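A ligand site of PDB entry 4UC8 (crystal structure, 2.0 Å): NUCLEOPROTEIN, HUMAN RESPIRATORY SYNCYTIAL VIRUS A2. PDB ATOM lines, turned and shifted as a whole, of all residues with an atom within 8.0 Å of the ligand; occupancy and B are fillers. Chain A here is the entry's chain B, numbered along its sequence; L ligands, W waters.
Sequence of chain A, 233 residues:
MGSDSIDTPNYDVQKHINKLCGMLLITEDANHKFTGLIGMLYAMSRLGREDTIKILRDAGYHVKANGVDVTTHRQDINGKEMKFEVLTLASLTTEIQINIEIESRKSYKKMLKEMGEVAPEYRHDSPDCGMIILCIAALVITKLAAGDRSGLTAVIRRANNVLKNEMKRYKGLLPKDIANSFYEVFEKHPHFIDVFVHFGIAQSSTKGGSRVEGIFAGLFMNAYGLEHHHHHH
Water W2 lies within hydrogen-bond range of O2 of the ligand and OE2 of Glu 117.
Water W3 lies within hydrogen-bond range of NE2 of His 124 and N1 of the ligand.
Water W1 lies within hydrogen-bond range of OE2 of Glu 101 (2.7 Å) and NZ of Lys 19 (3.2 Å).
The side-chain hydroxyl (OH) of Tyr 108 is in hydrogen-bond range of the side-chain carboxylate (OE1) of Glu 117 (2.7 Å).
The side-chain hydroxyl (OH) of Tyr 108 lies within hydrogen-bond range of the guanidinium group (NH1) of Arg 123 (2.8 Å).
NE of Arg 105 lies within salt-bridge range of OE2 of Glu 101 (3.0 Å).
The side-chain hydroxyl (OG) of Ser 104 is in hydrogen-bond range of the backbone carbonyl oxygen (O) of Met 23 (3.0 Å).
NH2 of Arg 123 is in salt-bridge range of OD2 of Asp 125, at 2.8 Å.
Merely in contact with the ligand: Arg 105 (3.4 Å), Tyr 108 (3.6 Å), Glu 101 (3.8 Å) and Ser 104 (3.9 Å).
Hydrophobic or aromatic side chains within 4 Å of the ligand: Tyr 108 and His 124.
The nearest printed residue that does not touch the ligand is Ile 26 (4.3 Å).
A ring nitrogen (NE2) of His 124 sits close to an oxygen (O1) of the ligand, 3.3 Å away.
The guanidinium group (NH2) of Arg 123 lies within salt-bridge range of an oxygen (O1) of the ligand.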
ATOM      1  N   LYS A  19     -23.528  -2.754 -31.746  1.00  0.00           N
ATOM      2  CA  LYS A  19     -23.977  -2.777 -30.348  1.00  0.00           C
ATOM      3  C   LYS A  19     -24.691  -1.464 -29.944  1.00  0.00           C
ATOM      4  O   LYS A  19     -25.641  -1.486 -29.160  1.00  0.00           O
ATOM      5  CB  LYS A  19     -22.807  -3.093 -29.411  1.00  0.00           C
ATOM      6  CG  LYS A  19     -23.193  -3.295 -27.924  1.00  0.00           C
ATOM      7  CD  LYS A  19     -22.221  -4.178 -27.152  1.00  0.00           C
ATOM      8  CE  LYS A  19     -20.998  -3.438 -26.659  1.00  0.00           C
ATOM      9  NZ  LYS A  19     -21.293  -2.534 -25.500  1.00  0.00           N
ATOM     10  N   GLY A  22     -28.007  -1.854 -31.375  1.00  0.00           N
ATOM     11  CA  GLY A  22     -28.682  -2.802 -30.504  1.00  0.00           C
ATOM     12  C   GLY A  22     -29.177  -2.186 -29.213  1.00  0.00           C
ATOM     13  O   GLY A  22     -30.261  -2.535 -28.738  1.00  0.00           O
ATOM     14  N   MET A  23     -28.379  -1.277 -28.637  1.00  0.00           N
ATOM     15  CA  MET A  23     -28.723  -0.571 -27.411  1.00  0.00           C
ATOM     16  C   MET A  23     -29.978   0.247 -27.569  1.00  0.00           C
ATOM     17  O   MET A  23     -30.830   0.233 -26.670  1.00  0.00           O
ATOM     18  CB  MET A  23     -27.552   0.272 -26.883  1.00  0.00           C
ATOM     19  CG  MET A  23     -26.490  -0.583 -26.233  1.00  0.00           C
ATOM     20  SD  MET A  23     -25.212   0.286 -25.323  1.00  0.00           S
ATOM     21  CE  MET A  23     -24.366   1.135 -26.615  1.00  0.00           C
ATOM     22  N   ILE A  26     -33.136  -2.177 -27.958  1.00  0.00           N
ATOM     23  CA  ILE A  26     -33.690  -2.771 -26.737  1.00  0.00           C
ATOM     24  C   ILE A  26     -34.334  -1.719 -25.824  1.00  0.00           C
ATOM     25  O   ILE A  26     -34.946  -2.096 -24.849  1.00  0.00           O
ATOM     26  CB  ILE A  26     -32.687  -3.683 -25.964  1.00  0.00           C
ATOM     27  CG1 ILE A  26     -31.573  -2.851 -25.263  1.00  0.00           C
ATOM     28  CG2 ILE A  26     -32.119  -4.797 -26.852  1.00  0.00           C
ATOM     29  CD1 ILE A  26     -30.991  -3.512 -23.978  1.00  0.00           C
ATOM     30  N   THR A  27     -34.191  -0.417 -26.138  1.00  0.00           N
ATOM     31  CA  THR A  27     -34.742   0.649 -25.300  1.00  0.00           C
ATOM     32  C   THR A  27     -36.211   0.875 -25.579  1.00  0.00           C
ATOM     33  O   THR A  27     -36.593   1.262 -26.685  1.00  0.00           O
ATOM     34  CB  THR A  27     -33.929   1.955 -25.416  1.00  0.00           C
ATOM     35  OG1 THR A  27     -32.539   1.658 -25.227  1.00  0.00           O
ATOM     36  CG2 THR A  27     -34.388   3.028 -24.402  1.00  0.00           C
ATOM     37  N   MET A  82     -18.519   3.870 -13.111  1.00  0.00           N
ATOM     38  CA  MET A  82     -18.722   2.985 -14.243  1.00  0.00           C
ATOM     39  C   MET A  82     -17.792   3.397 -15.398  1.00  0.00           C
ATOM     40  O   MET A  82     -17.558   4.584 -15.605  1.00  0.00           O
ATOM     41  CB  MET A  82     -20.182   3.019 -14.714  1.00  0.00           C
ATOM     42  CG  MET A  82     -21.124   2.250 -13.836  1.00  0.00           C
ATOM     43  SD  MET A  82     -22.536   1.619 -14.816  1.00  0.00           S
ATOM     44  CE  MET A  82     -21.787   0.185 -15.586  1.00  0.00           C
ATOM     45  N   PHE A  84     -17.233   3.386 -19.398  1.00  0.00           N
ATOM     46  CA  PHE A  84     -17.968   3.278 -20.670  1.00  0.00           C
ATOM     47  C   PHE A  84     -17.007   3.309 -21.868  1.00  0.00           C
ATOM     48  O   PHE A  84     -16.111   4.150 -21.928  1.00  0.00           O
ATOM     49  CB  PHE A  84     -18.995   4.412 -20.816  1.00  0.00           C
ATOM     50  CG  PHE A  84     -20.126   4.370 -19.810  1.00  0.00           C
ATOM     51  CD1 PHE A  84     -20.029   5.057 -18.602  1.00  0.00           C
ATOM     52  CD2 PHE A  84     -21.314   3.713 -20.100  1.00  0.00           C
ATOM     53  CE1 PHE A  84     -21.089   5.048 -17.673  1.00  0.00           C
ATOM     54  CE2 PHE A  84     -22.373   3.704 -19.171  1.00  0.00           C
ATOM     55  CZ  PHE A  84     -22.251   4.366 -17.968  1.00  0.00           C
ATOM     56  N   ILE A 100     -27.250   6.955 -24.229  1.00  0.00           N
ATOM     57  CA  ILE A 100     -27.853   5.861 -24.977  1.00  0.00           C
ATOM     58  C   ILE A 100     -27.644   4.555 -24.201  1.00  0.00           C
ATOM     59  O   ILE A 100     -28.604   3.810 -23.999  1.00  0.00           O
ATOM     60  CB  ILE A 100     -27.346   5.785 -26.456  1.00  0.00           C
ATOM     61  CG1 ILE A 100     -27.976   6.939 -27.282  1.00  0.00           C
ATOM     62  CG2 ILE A 100     -27.692   4.404 -27.068  1.00  0.00           C
ATOM     63  CD1 ILE A 100     -27.272   7.204 -28.641  1.00  0.00           C
ATOM     64  N   GLU A 101     -26.402   4.302 -23.721  1.00  0.00           N
ATOM     65  CA  GLU A 101     -26.090   3.109 -22.957  1.00  0.00           C
ATOM     66  C   GLU A 101     -26.847   3.069 -21.619  1.00  0.00           C
ATOM     67  O   GLU A 101     -27.369   2.005 -21.257  1.00  0.00           O
ATOM     68  CB  GLU A 101     -24.579   2.904 -22.748  1.00  0.00           C
ATOM     69  CG  GLU A 101     -24.271   1.624 -21.964  1.00  0.00           C
ATOM     70  CD  GLU A 101     -22.872   1.052 -21.963  1.00  0.00           C
ATOM     71  OE1 GLU A 101     -22.082   1.363 -22.898  1.00  0.00           O
ATOM     72  OE2 GLU A 101     -22.563   0.255 -21.046  1.00  0.00           O
ATOM     73  N   ILE A 102     -26.918   4.194 -20.910  1.00  0.00           N
ATOM     74  CA  ILE A 102     -27.607   4.259 -19.613  1.00  0.00           C
ATOM     75  C   ILE A 102     -29.083   3.892 -19.756  1.00  0.00           C
ATOM     76  O   ILE A 102     -29.577   3.086 -18.966  1.00  0.00           O
ATOM     77  CB  ILE A 102     -27.391   5.609 -18.873  1.00  0.00           C
ATOM     78  CG1 ILE A 102     -25.931   5.735 -18.386  1.00  0.00           C
ATOM     79  CG2 ILE A 102     -28.387   5.801 -17.697  1.00  0.00           C
ATOM     80  CD1 ILE A 102     -25.545   7.203 -17.940  1.00  0.00           C
ATOM     81  N   GLU A 103     -29.766   4.481 -20.761  1.00  0.00           N
ATOM     82  CA  GLU A 103     -31.181   4.228 -21.020  1.00  0.00           C
ATOM     83  C   GLU A 103     -31.426   2.780 -21.441  1.00  0.00           C
ATOM     84  O   GLU A 103     -32.407   2.182 -21.043  1.00  0.00           O
ATOM     85  CB  GLU A 103     -31.743   5.211 -22.066  1.00  0.00           C
ATOM     86  CG  GLU A 103     -31.849   6.644 -21.568  1.00  0.00           C
ATOM     87  CD  GLU A 103     -32.672   6.822 -20.298  1.00  0.00           C
ATOM     88  OE1 GLU A 103     -33.917   6.674 -20.379  1.00  0.00           O
ATOM     89  OE2 GLU A 103     -32.078   7.059 -19.224  1.00  0.00           O
ATOM     90  N   SER A 104     -30.479   2.221 -22.204  1.00  0.00           N
ATOM     91  CA  SER A 104     -30.481   0.838 -22.683  1.00  0.00           C
ATOM     92  C   SER A 104     -30.383  -0.122 -21.470  1.00  0.00           C
ATOM     93  O   SER A 104     -31.111  -1.104 -21.411  1.00  0.00           O
ATOM     94  CB  SER A 104     -29.289   0.624 -23.618  1.00  0.00           C
ATOM     95  OG  SER A 104     -29.360  -0.632 -24.233  1.00  0.00           O
ATOM     96  N   ARG A 105     -29.481   0.185 -20.509  1.00  0.00           N
ATOM     97  CA  ARG A 105     -29.300  -0.607 -19.281  1.00  0.00           C
ATOM     98  C   ARG A 105     -30.587  -0.640 -18.415  1.00  0.00           C
ATOM     99  O   ARG A 105     -30.883  -1.681 -17.807  1.00  0.00           O
ATOM    100  CB  ARG A 105     -28.120  -0.085 -18.454  1.00  0.00           C
ATOM    101  CG  ARG A 105     -26.764  -0.467 -19.047  1.00  0.00           C
ATOM    102  CD  ARG A 105     -25.646   0.196 -18.258  1.00  0.00           C
ATOM    103  NE  ARG A 105     -24.318  -0.250 -18.714  1.00  0.00           N
ATOM    104  CZ  ARG A 105     -23.670  -1.275 -18.184  1.00  0.00           C
ATOM    105  NH1 ARG A 105     -24.209  -1.982 -17.197  1.00  0.00           N
ATOM    106  NH2 ARG A 105     -22.477  -1.619 -18.659  1.00  0.00           N
ATOM    107  N   LYS A 106     -31.355   0.466 -18.367  1.00  0.00           N
ATOM    108  CA  LYS A 106     -32.615   0.561 -17.621  1.00  0.00           C
ATOM    109  C   LYS A 106     -33.661  -0.370 -18.229  1.00  0.00           C
ATOM    110  O   LYS A 106     -34.322  -1.100 -17.497  1.00  0.00           O
ATOM    111  CB  LYS A 106     -33.140   1.998 -17.596  1.00  0.00           C
ATOM    112  CG  LYS A 106     -32.302   2.928 -16.707  1.00  0.00           C
ATOM    113  CD  LYS A 106     -32.675   4.392 -16.916  1.00  0.00           C
ATOM    114  CE  LYS A 106     -31.886   5.299 -16.022  1.00  0.00           C
ATOM    115  NZ  LYS A 106     -32.150   6.732 -16.313  1.00  0.00           N
ATOM    116  N   SER A 107     -33.756  -0.386 -19.559  1.00  0.00           N
ATOM    117  CA  SER A 107     -34.659  -1.283 -20.292  1.00  0.00           C
ATOM    118  C   SER A 107     -34.218  -2.749 -20.144  1.00  0.00           C
ATOM    119  O   SER A 107     -35.072  -3.649 -20.063  1.00  0.00           O
ATOM    120  CB  SER A 107     -34.722  -0.902 -21.767  1.00  0.00           C
ATOM    121  OG  SER A 107     -35.551   0.230 -21.920  1.00  0.00           O
ATOM    122  N   TYR A 108     -32.885  -2.982 -20.115  1.00  0.00           N
ATOM    123  CA  TYR A 108     -32.311  -4.311 -19.953  1.00  0.00           C
ATOM    124  C   TYR A 108     -32.654  -4.892 -18.547  1.00  0.00           C
ATOM    125  O   TYR A 108     -32.962  -6.071 -18.426  1.00  0.00           O
ATOM    126  CB  TYR A 108     -30.790  -4.287 -20.171  1.00  0.00           C
ATOM    127  CG  TYR A 108     -30.196  -5.679 -20.363  1.00  0.00           C
ATOM    128  CD1 TYR A 108     -29.784  -6.434 -19.265  1.00  0.00           C
ATOM    129  CD2 TYR A 108     -30.051  -6.217 -21.633  1.00  0.00           C
ATOM    130  CE1 TYR A 108     -29.317  -7.744 -19.436  1.00  0.00           C
ATOM    131  CE2 TYR A 108     -29.517  -7.496 -21.820  1.00  0.00           C
ATOM    132  CZ  TYR A 108     -29.176  -8.266 -20.709  1.00  0.00           C
ATOM    133  OH  TYR A 108     -28.693  -9.535 -20.846  1.00  0.00           O
ATOM    134  N   LYS A 109     -32.652  -4.036 -17.502  1.00  0.00           N
ATOM    135  CA  LYS A 109     -33.028  -4.434 -16.141  1.00  0.00           C
ATOM    136  C   LYS A 109     -34.504  -4.882 -16.083  1.00  0.00           C
ATOM    137  O   LYS A 109     -34.825  -5.863 -15.411  1.00  0.00           O
ATOM    138  CB  LYS A 109     -32.756  -3.281 -15.145  1.00  0.00           C
ATOM    139  CG  LYS A 109     -32.992  -3.654 -13.670  1.00  0.00           C
ATOM    140  CD  LYS A 109     -32.912  -2.445 -12.775  1.00  0.00           C
ATOM    141  CE  LYS A 109     -33.179  -2.770 -11.322  1.00  0.00           C
ATOM    142  NZ  LYS A 109     -32.823  -1.626 -10.446  1.00  0.00           N
ATOM    143  N   MET A 111     -36.248  -6.161 -18.567  1.00  0.00           N
ATOM    144  CA  MET A 111     -36.254  -7.447 -19.294  1.00  0.00           C
ATOM    145  C   MET A 111     -35.815  -8.584 -18.364  1.00  0.00           C
ATOM    146  O   MET A 111     -36.473  -9.629 -18.337  1.00  0.00           O
ATOM    147  CB  MET A 111     -35.338  -7.371 -20.518  1.00  0.00           C
ATOM    148  CG  MET A 111     -35.997  -6.779 -21.725  1.00  0.00           C
ATOM    149  SD  MET A 111     -34.993  -7.035 -23.216  1.00  0.00           S
ATOM    150  CE  MET A 111     -33.807  -5.865 -22.990  1.00  0.00           C
ATOM    151  N   LEU A 112     -34.739  -8.358 -17.565  1.00  0.00           N
ATOM    152  CA  LEU A 112     -34.205  -9.291 -16.570  1.00  0.00           C
ATOM    153  C   LEU A 112     -35.272  -9.683 -15.553  1.00  0.00           C
ATOM    154  O   LEU A 112     -35.447 -10.863 -15.253  1.00  0.00           O
ATOM    155  CB  LEU A 112     -33.006  -8.699 -15.812  1.00  0.00           C
ATOM    156  CG  LEU A 112     -31.659  -8.664 -16.520  1.00  0.00           C
ATOM    157  CD1 LEU A 112     -30.583  -8.040 -15.598  1.00  0.00           C
ATOM    158  CD2 LEU A 112     -31.198 -10.078 -16.915  1.00  0.00           C
ATOM    159  N   GLU A 117     -32.072 -13.906 -17.386  1.00  0.00           N
ATOM    160  CA  GLU A 117     -31.096 -13.455 -18.395  1.00  0.00           C
ATOM    161  C   GLU A 117     -31.668 -13.520 -19.834  1.00  0.00           C
ATOM    162  O   GLU A 117     -32.499 -14.385 -20.137  1.00  0.00           O
ATOM    163  CB  GLU A 117     -29.740 -14.130 -18.248  1.00  0.00           C
ATOM    164  CG  GLU A 117     -28.821 -13.300 -17.349  1.00  0.00           C
ATOM    165  CD  GLU A 117     -28.341 -11.932 -17.831  1.00  0.00           C
ATOM    166  OE1 GLU A 117     -28.710 -11.488 -18.939  1.00  0.00           O
ATOM    167  OE2 GLU A 117     -27.600 -11.276 -17.050  1.00  0.00           O
ATOM    168  N   VAL A 118     -31.294 -12.542 -20.652  1.00  0.00           N
ATOM    169  CA  VAL A 118     -31.817 -12.316 -22.016  1.00  0.00           C
ATOM    170  C   VAL A 118     -31.091 -13.160 -23.077  1.00  0.00           C
ATOM    171  O   VAL A 118     -29.858 -13.149 -23.132  1.00  0.00           O
ATOM    172  CB  VAL A 118     -31.804 -10.788 -22.311  1.00  0.00           C
ATOM    173  CG1 VAL A 118     -32.396 -10.469 -23.672  1.00  0.00           C
ATOM    174  CG2 VAL A 118     -32.521 -10.016 -21.192  1.00  0.00           C
ATOM    175  N   ARG A 123     -30.913  -9.544 -27.362  1.00  0.00           N
ATOM    176  CA  ARG A 123     -29.885  -8.666 -26.790  1.00  0.00           C
ATOM    177  C   ARG A 123     -29.469  -7.565 -27.745  1.00  0.00           C
ATOM    178  O   ARG A 123     -29.666  -7.656 -28.962  1.00  0.00           O
ATOM    179  CB  ARG A 123     -28.650  -9.479 -26.359  1.00  0.00           C
ATOM    180  CG  ARG A 123     -28.800 -10.178 -25.022  1.00  0.00           C
ATOM    181  CD  ARG A 123     -27.610 -11.103 -24.742  1.00  0.00           C
ATOM    182  NE  ARG A 123     -26.339 -10.362 -24.784  1.00  0.00           N
ATOM    183  CZ  ARG A 123     -25.872  -9.627 -23.782  1.00  0.00           C
ATOM    184  NH1 ARG A 123     -26.546  -9.534 -22.640  1.00  0.00           N
ATOM    185  NH2 ARG A 123     -24.735  -8.977 -23.915  1.00  0.00           N
ATOM    186  N   HIS A 124     -28.826  -6.544 -27.178  1.00  0.00           N
ATOM    187  CA  HIS A 124     -28.293  -5.382 -27.856  1.00  0.00           C
ATOM    188  C   HIS A 124     -27.026  -5.726 -28.649  1.00  0.00           C
ATOM    189  O   HIS A 124     -26.583  -4.925 -29.467  1.00  0.00           O
ATOM    190  CB  HIS A 124     -27.988  -4.285 -26.816  1.00  0.00           C
ATOM    191  CG  HIS A 124     -27.126  -4.740 -25.685  1.00  0.00           C
ATOM    192  ND1 HIS A 124     -27.573  -5.708 -24.755  1.00  0.00           N
ATOM    193  CD2 HIS A 124     -25.852  -4.399 -25.388  1.00  0.00           C
ATOM    194  CE1 HIS A 124     -26.560  -5.909 -23.938  1.00  0.00           C
ATOM    195  NE2 HIS A 124     -25.500  -5.135 -24.271  1.00  0.00           N
ATOM    196  N   ASP A 125     -26.411  -6.888 -28.391  1.00  0.00           N
ATOM    197  CA  ASP A 125     -25.186  -7.253 -29.114  1.00  0.00           C
ATOM    198  C   ASP A 125     -25.418  -8.376 -30.160  1.00  0.00           C
ATOM    199  O   ASP A 125     -24.451  -8.982 -30.651  1.00  0.00           O
ATOM    200  CB  ASP A 125     -24.040  -7.595 -28.154  1.00  0.00           C
ATOM    201  CG  ASP A 125     -24.289  -8.763 -27.194  1.00  0.00           C
ATOM    202  OD1 ASP A 125     -25.365  -9.413 -27.297  1.00  0.00           O
ATOM    203  OD2 ASP A 125     -23.413  -9.020 -26.336  1.00  0.00           O
HETATM  204  N1  LIG L   1     -22.812  -5.772 -20.090  1.00  0.00           N
HETATM  205  C1  LIG L   1     -24.091  -6.315 -19.601  1.00  0.00           C
HETATM  206  C2  LIG L   1     -24.725  -7.249 -20.643  1.00  0.00           C
HETATM  207  O1  LIG L   1     -24.428  -7.077 -21.854  1.00  0.00           O
HETATM  208  C3  LIG L   1     -25.086  -5.185 -19.172  1.00  0.00           C
HETATM  209  C4  LIG L   1     -25.576  -4.240 -20.257  1.00  0.00           C
HETATM  210  C5  LIG L   1     -24.741  -3.239 -20.768  1.00  0.00           C
HETATM  211  C6  LIG L   1     -26.882  -4.321 -20.732  1.00  0.00           C
HETATM  212  C7  LIG L   1     -25.201  -2.362 -21.769  1.00  0.00           C
HETATM  213  C8  LIG L   1     -27.338  -3.427 -21.715  1.00  0.00           C
HETATM  214  C9  LIG L   1     -26.492  -2.469 -22.240  1.00  0.00           C
HETATM  215  O2  LIG L   1     -25.468  -8.165 -20.245  1.00  0.00           O
HETATM  216  O   HOH W   1     -21.939  -2.059 -22.383  1.00  0.00           O
HETATM  217  O   HOH W   2     -25.935  -8.878 -17.693  1.00  0.00           O
HETATM  218  O   HOH W   3     -22.695  -4.581 -22.991  1.00  0.00           O
